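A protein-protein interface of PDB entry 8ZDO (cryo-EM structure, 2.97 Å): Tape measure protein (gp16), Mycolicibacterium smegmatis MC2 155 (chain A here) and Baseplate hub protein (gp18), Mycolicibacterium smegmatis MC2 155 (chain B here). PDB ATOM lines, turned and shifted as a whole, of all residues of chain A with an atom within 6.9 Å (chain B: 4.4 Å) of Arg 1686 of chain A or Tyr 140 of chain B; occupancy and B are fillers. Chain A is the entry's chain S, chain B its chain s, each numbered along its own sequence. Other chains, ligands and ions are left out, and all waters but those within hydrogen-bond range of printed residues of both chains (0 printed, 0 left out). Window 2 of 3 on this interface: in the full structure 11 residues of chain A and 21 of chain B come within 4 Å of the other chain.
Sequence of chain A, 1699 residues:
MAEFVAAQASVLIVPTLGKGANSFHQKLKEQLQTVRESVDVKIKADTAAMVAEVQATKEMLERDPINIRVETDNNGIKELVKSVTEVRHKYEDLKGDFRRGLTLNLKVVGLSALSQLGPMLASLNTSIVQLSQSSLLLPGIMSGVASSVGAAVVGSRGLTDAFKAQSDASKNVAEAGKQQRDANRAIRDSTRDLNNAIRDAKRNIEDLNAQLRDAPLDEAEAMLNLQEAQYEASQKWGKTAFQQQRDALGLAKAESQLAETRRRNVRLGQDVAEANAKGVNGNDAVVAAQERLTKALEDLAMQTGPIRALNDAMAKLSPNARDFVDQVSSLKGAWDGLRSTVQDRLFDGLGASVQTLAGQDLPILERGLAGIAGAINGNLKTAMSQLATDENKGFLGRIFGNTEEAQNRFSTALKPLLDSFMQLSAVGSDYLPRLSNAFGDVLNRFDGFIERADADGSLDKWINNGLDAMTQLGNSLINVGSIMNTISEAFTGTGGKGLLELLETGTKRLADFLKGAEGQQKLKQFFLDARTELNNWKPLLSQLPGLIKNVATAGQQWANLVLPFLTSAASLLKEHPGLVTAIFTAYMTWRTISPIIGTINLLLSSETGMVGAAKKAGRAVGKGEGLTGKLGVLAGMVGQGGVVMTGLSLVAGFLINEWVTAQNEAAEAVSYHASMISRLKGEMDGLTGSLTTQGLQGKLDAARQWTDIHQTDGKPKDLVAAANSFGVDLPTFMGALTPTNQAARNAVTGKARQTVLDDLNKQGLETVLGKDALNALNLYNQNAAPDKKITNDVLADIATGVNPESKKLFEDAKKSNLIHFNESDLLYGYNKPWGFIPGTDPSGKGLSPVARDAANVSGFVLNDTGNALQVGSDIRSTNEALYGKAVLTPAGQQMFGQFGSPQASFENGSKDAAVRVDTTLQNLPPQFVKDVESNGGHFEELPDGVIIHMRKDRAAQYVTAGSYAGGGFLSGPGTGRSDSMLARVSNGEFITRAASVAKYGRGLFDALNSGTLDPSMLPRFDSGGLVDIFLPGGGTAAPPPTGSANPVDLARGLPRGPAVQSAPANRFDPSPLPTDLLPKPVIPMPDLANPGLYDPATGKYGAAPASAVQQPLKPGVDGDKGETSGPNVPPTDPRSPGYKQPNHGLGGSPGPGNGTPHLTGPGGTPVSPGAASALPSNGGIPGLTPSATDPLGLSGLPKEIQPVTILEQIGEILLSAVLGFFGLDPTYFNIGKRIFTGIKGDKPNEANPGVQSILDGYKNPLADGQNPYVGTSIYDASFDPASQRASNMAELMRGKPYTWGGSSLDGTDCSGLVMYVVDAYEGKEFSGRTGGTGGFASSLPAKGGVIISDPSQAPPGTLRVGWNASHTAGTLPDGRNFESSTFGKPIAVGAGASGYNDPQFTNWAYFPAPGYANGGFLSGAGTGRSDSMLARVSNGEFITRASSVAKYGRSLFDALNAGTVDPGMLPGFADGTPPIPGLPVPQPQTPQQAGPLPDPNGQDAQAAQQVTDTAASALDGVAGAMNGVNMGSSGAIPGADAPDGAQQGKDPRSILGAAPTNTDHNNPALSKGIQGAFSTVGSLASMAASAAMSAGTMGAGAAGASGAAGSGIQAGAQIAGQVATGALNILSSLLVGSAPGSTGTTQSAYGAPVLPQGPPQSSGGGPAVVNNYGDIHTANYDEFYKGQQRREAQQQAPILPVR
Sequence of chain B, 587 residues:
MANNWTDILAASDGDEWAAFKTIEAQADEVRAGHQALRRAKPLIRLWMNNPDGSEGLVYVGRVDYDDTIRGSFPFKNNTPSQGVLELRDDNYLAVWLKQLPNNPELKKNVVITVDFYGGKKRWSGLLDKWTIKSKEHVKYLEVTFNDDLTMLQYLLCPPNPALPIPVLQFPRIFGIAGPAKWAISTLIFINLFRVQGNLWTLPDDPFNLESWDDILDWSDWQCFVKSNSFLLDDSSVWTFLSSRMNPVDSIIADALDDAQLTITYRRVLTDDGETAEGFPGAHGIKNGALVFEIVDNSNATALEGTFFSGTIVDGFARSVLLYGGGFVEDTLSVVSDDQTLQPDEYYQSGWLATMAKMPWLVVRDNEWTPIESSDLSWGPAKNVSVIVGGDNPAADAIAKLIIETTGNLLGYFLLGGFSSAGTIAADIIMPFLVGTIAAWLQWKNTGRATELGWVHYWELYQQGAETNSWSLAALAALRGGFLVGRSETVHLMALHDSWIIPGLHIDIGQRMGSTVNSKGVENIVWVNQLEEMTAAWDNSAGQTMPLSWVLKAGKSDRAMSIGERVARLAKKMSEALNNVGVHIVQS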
ATOM      1  N   ASP A1678     -25.020  18.855   1.931  1.00  0.00           N
ATOM      2  CA  ASP A1678     -24.702  18.938   0.512  1.00  0.00           C
ATOM      3  C   ASP A1678     -24.321  20.357   0.108  1.00  0.00           C
ATOM      4  O   ASP A1678     -23.273  20.573  -0.513  1.00  0.00           O
ATOM      5  CB  ASP A1678     -25.884  18.432  -0.317  1.00  0.00           C
ATOM      6  CG  ASP A1678     -25.540  18.265  -1.787  1.00  0.00           C
ATOM      7  OD1 ASP A1678     -24.784  17.328  -2.118  1.00  0.00           O
ATOM      8  OD2 ASP A1678     -26.035  19.062  -2.611  1.00  0.00           O
ATOM      9  N   GLU A1679     -25.145  21.346   0.469  1.00  0.00           N
ATOM     10  CA  GLU A1679     -24.827  22.709   0.062  1.00  0.00           C
ATOM     11  C   GLU A1679     -23.642  23.255   0.844  1.00  0.00           C
ATOM     12  O   GLU A1679     -22.906  24.096   0.326  1.00  0.00           O
ATOM     13  CB  GLU A1679     -26.036  23.635   0.218  1.00  0.00           C
ATOM     14  CG  GLU A1679     -26.380  24.033   1.640  1.00  0.00           C
ATOM     15  CD  GLU A1679     -25.721  25.341   2.049  1.00  0.00           C
ATOM     16  OE1 GLU A1679     -25.301  26.101   1.149  1.00  0.00           O
ATOM     17  OE2 GLU A1679     -25.614  25.603   3.268  1.00  0.00           O
ATOM     18  N   PHE A1680     -23.442  22.801   2.083  1.00  0.00           N
ATOM     19  CA  PHE A1680     -22.269  23.226   2.838  1.00  0.00           C
ATOM     20  C   PHE A1680     -20.989  22.740   2.170  1.00  0.00           C
ATOM     21  O   PHE A1680     -20.027  23.502   2.006  1.00  0.00           O
ATOM     22  CB  PHE A1680     -22.351  22.715   4.276  1.00  0.00           C
ATOM     23  CG  PHE A1680     -21.262  23.240   5.166  1.00  0.00           C
ATOM     24  CD1 PHE A1680     -21.424  24.435   5.843  1.00  0.00           C
ATOM     25  CD2 PHE A1680     -20.074  22.546   5.319  1.00  0.00           C
ATOM     26  CE1 PHE A1680     -20.429  24.925   6.658  1.00  0.00           C
ATOM     27  CE2 PHE A1680     -19.073  23.033   6.131  1.00  0.00           C
ATOM     28  CZ  PHE A1680     -19.251  24.223   6.803  1.00  0.00           C
ATOM     29  N   TYR A1681     -20.966  21.468   1.766  1.00  0.00           N
ATOM     30  CA  TYR A1681     -19.803  20.940   1.062  1.00  0.00           C
ATOM     31  C   TYR A1681     -19.615  21.637  -0.278  1.00  0.00           C
ATOM     32  O   TYR A1681     -18.485  21.948  -0.672  1.00  0.00           O
ATOM     33  CB  TYR A1681     -19.947  19.431   0.872  1.00  0.00           C
ATOM     34  CG  TYR A1681     -18.663  18.746   0.472  1.00  0.00           C
ATOM     35  CD1 TYR A1681     -17.735  18.361   1.427  1.00  0.00           C
ATOM     36  CD2 TYR A1681     -18.380  18.486  -0.860  1.00  0.00           C
ATOM     37  CE1 TYR A1681     -16.560  17.737   1.067  1.00  0.00           C
ATOM     38  CE2 TYR A1681     -17.207  17.860  -1.230  1.00  0.00           C
ATOM     39  CZ  TYR A1681     -16.301  17.488  -0.262  1.00  0.00           C
ATOM     40  OH  TYR A1681     -15.129  16.865  -0.625  1.00  0.00           O
ATOM     41  N   LYS A1682     -20.714  21.898  -0.991  1.00  0.00           N
ATOM     42  CA  LYS A1682     -20.612  22.586  -2.273  1.00  0.00           C
ATOM     43  C   LYS A1682     -20.086  24.006  -2.102  1.00  0.00           C
ATOM     44  O   LYS A1682     -19.302  24.485  -2.923  1.00  0.00           O
ATOM     45  CB  LYS A1682     -21.969  22.592  -2.977  1.00  0.00           C
ATOM     46  CG  LYS A1682     -22.367  21.244  -3.556  1.00  0.00           C
ATOM     47  CD  LYS A1682     -23.600  21.357  -4.438  1.00  0.00           C
ATOM     48  CE  LYS A1682     -24.821  21.763  -3.634  1.00  0.00           C
ATOM     49  NZ  LYS A1682     -26.059  21.763  -4.463  1.00  0.00           N
ATOM     50  N   GLY A1683     -20.511  24.697  -1.043  1.00  0.00           N
ATOM     51  CA  GLY A1683     -20.012  26.037  -0.792  1.00  0.00           C
ATOM     52  C   GLY A1683     -18.545  26.051  -0.412  1.00  0.00           C
ATOM     53  O   GLY A1683     -17.793  26.933  -0.836  1.00  0.00           O
ATOM     54  N   GLN A1684     -18.117  25.082   0.400  1.00  0.00           N
ATOM     55  CA  GLN A1684     -16.696  24.968   0.706  1.00  0.00           C
ATOM     56  C   GLN A1684     -15.887  24.706  -0.557  1.00  0.00           C
ATOM     57  O   GLN A1684     -14.823  25.305  -0.763  1.00  0.00           O
ATOM     58  CB  GLN A1684     -16.464  23.861   1.733  1.00  0.00           C
ATOM     59  CG  GLN A1684     -16.971  24.184   3.127  1.00  0.00           C
ATOM     60  CD  GLN A1684     -16.418  25.489   3.668  1.00  0.00           C
ATOM     61  OE1 GLN A1684     -17.138  26.271   4.285  1.00  0.00           O
ATOM     62  NE2 GLN A1684     -15.130  25.726   3.446  1.00  0.00           N
ATOM     63  N   GLN A1685     -16.387  23.821  -1.422  1.00  0.00           N
ATOM     64  CA  GLN A1685     -15.706  23.550  -2.681  1.00  0.00           C
ATOM     65  C   GLN A1685     -15.672  24.786  -3.569  1.00  0.00           C
ATOM     66  O   GLN A1685     -14.675  25.037  -4.248  1.00  0.00           O
ATOM     67  CB  GLN A1685     -16.384  22.387  -3.406  1.00  0.00           C
ATOM     68  CG  GLN A1685     -16.191  21.040  -2.733  1.00  0.00           C
ATOM     69  CD  GLN A1685     -14.837  20.908  -2.069  1.00  0.00           C
ATOM     70  OE1 GLN A1685     -14.703  21.099  -0.861  1.00  0.00           O
ATOM     71  NE2 GLN A1685     -13.823  20.578  -2.858  1.00  0.00           N
ATOM     72  N   ARG A1686     -16.755  25.564  -3.582  1.00  0.00           N
ATOM     73  CA  ARG A1686     -16.782  26.791  -4.372  1.00  0.00           C
ATOM     74  C   ARG A1686     -15.776  27.807  -3.855  1.00  0.00           C
ATOM     75  O   ARG A1686     -15.107  28.482  -4.644  1.00  0.00           O
ATOM     76  CB  ARG A1686     -18.187  27.388  -4.374  1.00  0.00           C
ATOM     77  CG  ARG A1686     -19.075  26.905  -5.504  1.00  0.00           C
ATOM     78  CD  ARG A1686     -20.480  27.462  -5.364  1.00  0.00           C
ATOM     79  NE  ARG A1686     -21.167  26.916  -4.199  1.00  0.00           N
ATOM     80  CZ  ARG A1686     -22.283  27.413  -3.685  1.00  0.00           C
ATOM     81  NH1 ARG A1686     -22.867  28.480  -4.204  1.00  0.00           N
ATOM     82  NH2 ARG A1686     -22.825  26.825  -2.622  1.00  0.00           N
ATOM     83  N   ARG A1687     -15.661  27.943  -2.534  1.00  0.00           N
ATOM     84  CA  ARG A1687     -14.679  28.864  -1.972  1.00  0.00           C
ATOM     85  C   ARG A1687     -13.256  28.425  -2.302  1.00  0.00           C
ATOM     86  O   ARG A1687     -12.414  29.249  -2.683  1.00  0.00           O
ATOM     87  CB  ARG A1687     -14.876  28.978  -0.462  1.00  0.00           C
ATOM     88  CG  ARG A1687     -16.020  29.892  -0.070  1.00  0.00           C
ATOM     89  CD  ARG A1687     -16.027  30.179   1.421  1.00  0.00           C
ATOM     90  NE  ARG A1687     -16.912  29.277   2.148  1.00  0.00           N
ATOM     91  CZ  ARG A1687     -17.046  29.263   3.467  1.00  0.00           C
ATOM     92  NH1 ARG A1687     -16.354  30.084   4.240  1.00  0.00           N
ATOM     93  NH2 ARG A1687     -17.895  28.406   4.024  1.00  0.00           N
ATOM     94  N   GLU A1688     -12.972  27.125  -2.183  1.00  0.00           N
ATOM     95  CA  GLU A1688     -11.646  26.632  -2.541  1.00  0.00           C
ATOM     96  C   GLU A1688     -11.373  26.814  -4.030  1.00  0.00           C
ATOM     97  O   GLU A1688     -10.246  27.130  -4.429  1.00  0.00           O
ATOM     98  CB  GLU A1688     -11.502  25.165  -2.142  1.00  0.00           C
ATOM     99  CG  GLU A1688     -11.713  24.901  -0.662  1.00  0.00           C
ATOM    100  CD  GLU A1688     -10.418  24.899   0.121  1.00  0.00           C
ATOM    101  OE1 GLU A1688      -9.350  24.705  -0.496  1.00  0.00           O
ATOM    102  OE2 GLU A1688     -10.467  25.091   1.353  1.00  0.00           O
ATOM    103  N   ALA A1689     -12.389  26.604  -4.869  1.00  0.00           N
ATOM    104  CA  ALA A1689     -12.234  26.805  -6.303  1.00  0.00           C
ATOM    105  C   ALA A1689     -11.973  28.267  -6.630  1.00  0.00           C
ATOM    106  O   ALA A1689     -11.180  28.575  -7.523  1.00  0.00           O
ATOM    107  CB  ALA A1689     -13.474  26.304  -7.038  1.00  0.00           C
ATOM    108  N   GLN A1690     -12.643  29.181  -5.929  1.00  0.00           N
ATOM    109  CA  GLN A1690     -12.362  30.598  -6.113  1.00  0.00           C
ATOM    110  C   GLN A1690     -10.931  30.921  -5.716  1.00  0.00           C
ATOM    111  O   GLN A1690     -10.250  31.700  -6.390  1.00  0.00           O
ATOM    112  CB  GLN A1690     -13.347  31.436  -5.301  1.00  0.00           C
ATOM    113  CG  GLN A1690     -13.038  32.917  -5.289  1.00  0.00           C
ATOM    114  CD  GLN A1690     -14.195  33.740  -4.775  1.00  0.00           C
ATOM    115  OE1 GLN A1690     -15.243  33.204  -4.423  1.00  0.00           O
ATOM    116  NE2 GLN A1690     -14.013  35.052  -4.727  1.00  0.00           N
ATOM    117  N   GLN A1691     -10.459  30.328  -4.619  1.00  0.00           N
ATOM    118  CA  GLN A1691      -9.099  30.594  -4.168  1.00  0.00           C
ATOM    119  C   GLN A1691      -8.059  30.063  -5.150  1.00  0.00           C
ATOM    120  O   GLN A1691      -7.068  30.743  -5.436  1.00  0.00           O
ATOM    121  CB  GLN A1691      -8.881  29.989  -2.783  1.00  0.00           C
ATOM    122  CG  GLN A1691      -7.533  30.321  -2.171  1.00  0.00           C
ATOM    123  CD  GLN A1691      -7.403  31.786  -1.816  1.00  0.00           C
ATOM    124  OE1 GLN A1691      -8.387  32.442  -1.470  1.00  0.00           O
ATOM    125  NE2 GLN A1691      -6.187  32.310  -1.903  1.00  0.00           N
ATOM    126  N   ILE B  69     -27.794  38.133  -5.578  1.00  0.00           N
ATOM    127  CA  ILE B  69     -28.004  37.085  -4.587  1.00  0.00           C
ATOM    128  C   ILE B  69     -26.780  36.930  -3.698  1.00  0.00           C
ATOM    129  O   ILE B  69     -26.901  36.803  -2.478  1.00  0.00           O
ATOM    130  CB  ILE B  69     -28.359  35.758  -5.288  1.00  0.00           C
ATOM    131  CG1 ILE B  69     -29.828  35.742  -5.702  1.00  0.00           C
ATOM    132  CG2 ILE B  69     -28.049  34.571  -4.394  1.00  0.00           C
ATOM    133  CD1 ILE B  69     -30.213  34.516  -6.481  1.00  0.00           C
ATOM    134  N   ARG B  70     -25.596  36.957  -4.299  1.00  0.00           N
ATOM    135  CA  ARG B  70     -24.350  36.708  -3.597  1.00  0.00           C
ATOM    136  C   ARG B  70     -23.240  37.438  -4.335  1.00  0.00           C
ATOM    137  O   ARG B  70     -23.351  37.714  -5.530  1.00  0.00           O
ATOM    138  CB  ARG B  70     -24.078  35.204  -3.518  1.00  0.00           C
ATOM    139  CG  ARG B  70     -22.802  34.791  -2.832  1.00  0.00           C
ATOM    140  CD  ARG B  70     -22.823  33.300  -2.604  1.00  0.00           C
ATOM    141  NE  ARG B  70     -24.095  32.889  -2.027  1.00  0.00           N
ATOM    142  CZ  ARG B  70     -24.435  31.634  -1.766  1.00  0.00           C
ATOM    143  NH1 ARG B  70     -23.612  30.630  -2.016  1.00  0.00           N
ATOM    144  NH2 ARG B  70     -25.632  31.382  -1.243  1.00  0.00           N
ATOM    145  N   GLU B  86     -23.691  36.203  -8.033  1.00  0.00           N
ATOM    146  CA  GLU B  86     -24.843  35.335  -8.229  1.00  0.00           C
ATOM    147  C   GLU B  86     -26.090  36.176  -8.453  1.00  0.00           C
ATOM    148  O   GLU B  86     -26.391  37.074  -7.661  1.00  0.00           O
ATOM    149  CB  GLU B  86     -25.037  34.399  -7.036  1.00  0.00           C
ATOM    150  CG  GLU B  86     -24.011  33.285  -6.966  1.00  0.00           C
ATOM    151  CD  GLU B  86     -24.247  32.346  -5.801  1.00  0.00           C
ATOM    152  OE1 GLU B  86     -25.237  32.547  -5.067  1.00  0.00           O
ATOM    153  OE2 GLU B  86     -23.443  31.407  -5.620  1.00  0.00           O
ATOM    154  N   LEU B  87     -26.812  35.878  -9.530  1.00  0.00           N
ATOM    155  CA  LEU B  87     -28.019  36.595  -9.901  1.00  0.00           C
ATOM    156  C   LEU B  87     -29.163  35.608 -10.059  1.00  0.00           C
ATOM    157  O   LEU B  87     -28.952  34.404 -10.213  1.00  0.00           O
ATOM    158  CB  LEU B  87     -27.827  37.379 -11.206  1.00  0.00           C
ATOM    159  CG  LEU B  87     -26.556  38.218 -11.322  1.00  0.00           C
ATOM    160  CD1 LEU B  87     -26.393  38.754 -12.730  1.00  0.00           C
ATOM    161  CD2 LEU B  87     -26.591  39.352 -10.321  1.00  0.00           C
ATOM    162  N   ASP B  89     -32.368  34.164 -12.295  1.00  0.00           N
ATOM    163  CA  ASP B  89     -32.456  33.918 -13.732  1.00  0.00           C
ATOM    164  C   ASP B  89     -33.230  35.015 -14.452  1.00  0.00           C
ATOM    165  O   ASP B  89     -32.842  35.440 -15.545  1.00  0.00           O
ATOM    166  CB  ASP B  89     -33.095  32.559 -14.006  1.00  0.00           C
ATOM    167  CG  ASP B  89     -32.068  31.466 -14.202  1.00  0.00           C
ATOM    168  OD1 ASP B  89     -30.885  31.786 -14.436  1.00  0.00           O
ATOM    169  OD2 ASP B  89     -32.451  30.282 -14.157  1.00  0.00           O
ATOM    170  N   THR B 131     -22.632  29.784 -14.904  1.00  0.00           N
ATOM    171  CA  THR B 131     -23.228  28.478 -14.683  1.00  0.00           C
ATOM    172  C   THR B 131     -24.652  28.666 -14.192  1.00  0.00           C
ATOM    173  O   THR B 131     -24.886  29.409 -13.235  1.00  0.00           O
ATOM    174  CB  THR B 131     -22.424  27.664 -13.663  1.00  0.00           C
ATOM    175  OG1 THR B 131     -21.051  27.615 -14.064  1.00  0.00           O
ATOM    176  CG2 THR B 131     -22.960  26.250 -13.563  1.00  0.00           C
ATOM    177  N   ILE B 132     -25.594  28.001 -14.850  1.00  0.00           N
ATOM    178  CA  ILE B 132     -26.967  27.939 -14.366  1.00  0.00           C
ATOM    179  C   ILE B 132     -27.046  26.822 -13.335  1.00  0.00           C
ATOM    180  O   ILE B 132     -26.821  25.652 -13.657  1.00  0.00           O
ATOM    181  CB  ILE B 132     -27.953  27.704 -15.516  1.00  0.00           C
ATOM    182  CG1 ILE B 132     -27.706  28.706 -16.641  1.00  0.00           C
ATOM    183  CG2 ILE B 132     -29.378  27.802 -15.016  1.00  0.00           C
ATOM    184  CD1 ILE B 132     -28.529  28.448 -17.870  1.00  0.00           C
ATOM    185  N   LYS B 133     -27.361  27.178 -12.097  1.00  0.00           N
ATOM    186  CA  LYS B 133     -27.367  26.238 -10.989  1.00  0.00           C
ATOM    187  C   LYS B 133     -28.749  26.187 -10.362  1.00  0.00           C
ATOM    188  O   LYS B 133     -29.413  27.215 -10.208  1.00  0.00           O
ATOM    189  CB  LYS B 133     -26.329  26.623  -9.935  1.00  0.00           C
ATOM    190  CG  LYS B 133     -24.897  26.462 -10.401  1.00  0.00           C
ATOM    191  CD  LYS B 133     -23.918  26.733  -9.277  1.00  0.00           C
ATOM    192  CE  LYS B 133     -22.505  26.354  -9.679  1.00  0.00           C
ATOM    193  NZ  LYS B 133     -21.535  26.589  -8.576  1.00  0.00           N
ATOM    194  N   LYS B 135     -30.975  25.082  -7.061  1.00  0.00           N
ATOM    195  CA  LYS B 135     -31.166  24.683  -5.672  1.00  0.00           C
ATOM    196  C   LYS B 135     -32.663  24.516  -5.444  1.00  0.00           C
ATOM    197  O   LYS B 135     -33.417  25.494  -5.496  1.00  0.00           O
ATOM    198  CB  LYS B 135     -30.567  25.708  -4.709  1.00  0.00           C
ATOM    199  CG  LYS B 135     -30.836  27.161  -5.073  1.00  0.00           C
ATOM    200  CD  LYS B 135     -30.187  28.104  -4.071  1.00  0.00           C
ATOM    201  CE  LYS B 135     -30.926  29.431  -3.991  1.00  0.00           C
ATOM    202  NZ  LYS B 135     -31.095  30.062  -5.328  1.00  0.00           N
ATOM    203  N   VAL B 138     -34.964  25.705  -7.968  1.00  0.00           N
ATOM    204  CA  VAL B 138     -34.863  27.151  -8.113  1.00  0.00           C
ATOM    205  C   VAL B 138     -33.561  27.456  -8.833  1.00  0.00           C
ATOM    206  O   VAL B 138     -32.480  27.123  -8.341  1.00  0.00           O
ATOM    207  CB  VAL B 138     -34.919  27.854  -6.749  1.00  0.00           C
ATOM    208  CG1 VAL B 138     -34.704  29.331  -6.921  1.00  0.00           C
ATOM    209  CG2 VAL B 138     -36.247  27.586  -6.077  1.00  0.00           C
ATOM    210  N   LYS B 139     -33.653  28.098  -9.991  1.00  0.00           N
ATOM    211  CA  LYS B 139     -32.503  28.271 -10.865  1.00  0.00           C
ATOM    212  C   LYS B 139     -31.969  29.692 -10.772  1.00  0.00           C
ATOM    213  O   LYS B 139     -32.732  30.658 -10.861  1.00  0.00           O
ATOM    214  CB  LYS B 139     -32.873  27.930 -12.308  1.00  0.00           C
ATOM    215  CG  LYS B 139     -33.146  26.458 -12.529  1.00  0.00           C
ATOM    216  CD  LYS B 139     -33.223  26.119 -14.001  1.00  0.00           C
ATOM    217  CE  LYS B 139     -33.346  24.620 -14.197  1.00  0.00           C
ATOM    218  NZ  LYS B 139     -33.592  24.255 -15.616  1.00  0.00           N
ATOM    219  N   TYR B 140     -30.658  29.807 -10.581  1.00  0.00           N
ATOM    220  CA  TYR B 140     -29.956  31.079 -10.572  1.00  0.00           C
ATOM    221  C   TYR B 140     -28.721  30.958 -11.454  1.00  0.00           C
ATOM    222  O   TYR B 140     -28.386  29.878 -11.945  1.00  0.00           O
ATOM    223  CB  TYR B 140     -29.572  31.503  -9.148  1.00  0.00           C
ATOM    224  CG  TYR B 140     -28.607  30.569  -8.461  1.00  0.00           C
ATOM    225  CD1 TYR B 140     -29.055  29.427  -7.820  1.00  0.00           C
ATOM    226  CD2 TYR B 140     -27.247  30.837  -8.447  1.00  0.00           C
ATOM    227  CE1 TYR B 140     -28.179  28.573  -7.192  1.00  0.00           C
ATOM    228  CE2 TYR B 140     -26.362  29.990  -7.821  1.00  0.00           C
ATOM    229  CZ  TYR B 140     -26.833  28.858  -7.195  1.00  0.00           C
ATOM    230  OH  TYR B 140     -25.954  28.007  -6.566  1.00  0.00           O
ATOM    231  N   LEU B 141     -28.045  32.082 -11.669  1.00  0.00           N
ATOM    232  CA  LEU B 141     -26.861  32.134 -12.514  1.00  0.00           C
ATOM    233  C   LEU B 141     -25.687  32.619 -11.682  1.00  0.00           C
ATOM    234  O   LEU B 141     -25.733  33.721 -11.126  1.00  0.00           O
ATOM    235  CB  LEU B 141     -27.089  33.057 -13.711  1.00  0.00           C
ATOM    236  CG  LEU B 141     -26.027  33.054 -14.807  1.00  0.00           C
ATOM    237  CD1 LEU B 141     -26.288  31.933 -15.778  1.00  0.00           C
ATOM    238  CD2 LEU B 141     -26.003  34.380 -15.530  1.00  0.00           C
ATOM    239  N   GLU B 142     -24.637  31.808 -11.596  1.00  0.00           N
ATOM    240  CA  GLU B 142     -23.408  32.214 -10.931  1.00  0.00           C
ATOM    241  C   GLU B 142     -22.384  32.573 -11.995  1.00  0.00           C
ATOM    242  O   GLU B 142     -22.165  31.810 -12.938  1.00  0.00           O
ATOM    243  CB  GLU B 142     -22.883  31.120  -9.997  1.00  0.00           C
ATOM    244  CG  GLU B 142     -22.304  29.885 -10.668  1.00  0.00           C
ATOM    245  CD  GLU B 142     -20.800  29.985 -10.859  1.00  0.00           C
ATOM    246  OE1 GLU B 142     -20.160  30.768 -10.125  1.00  0.00           O
ATOM    247  OE2 GLU B 142     -20.257  29.292 -11.745  1.00  0.00           O
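NH1 of Arg 1686 of chain A sits close to NH1 of Arg 70 of chain B (3.2 Å). NH1 of Arg 1686 of chain A is in salt-bridge range of OE2 of Glu 86 of chain B (3.3 Å).
The backbone carbonyl oxygen of Lys 1682 of chain A sits at hydrogen-bond distance from the guanidinium group of Arg 1686 of chain A (3.3 Å). N of Ile 69 of chain B lies within hydrogen-bond range of O of Glu 86 of chain B (2.7 Å). O of Tyr 140 of chain B is in hydrogen-bond range of N of Lys 133 of chain B. OE1 of Glu 86 of chain B is in salt-bridge range of NE of Arg 70 of chain B (3.3 Å).
Among the printed residues, merely in contact across the chains: Arg 1686 of chain A with Lys 133 of chain B and Arg 1686 of chain A with Tyr 140 of chain B.
Printed residues of chain A within 4 Å of Tyr 140 of chain B: Arg 1686. Of the printed residues of chain A, Glu 86 of chain B touches Arg 1686. Of the printed residues of chain A, Arg 70 of chain B touches Arg 1686 (3.2 Å). Of the printed residues of chain A, Lys 133 of chain B touches Arg 1686 (3.5 Å). The nearest printed residue of chain A that does not touch Arg 70 of chain B is Glu 1679 of chain A (5.8 Å).
Hydrophobic or aromatic side chains of chain B within 4 Å of the printed part of chain A: Tyr 140.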
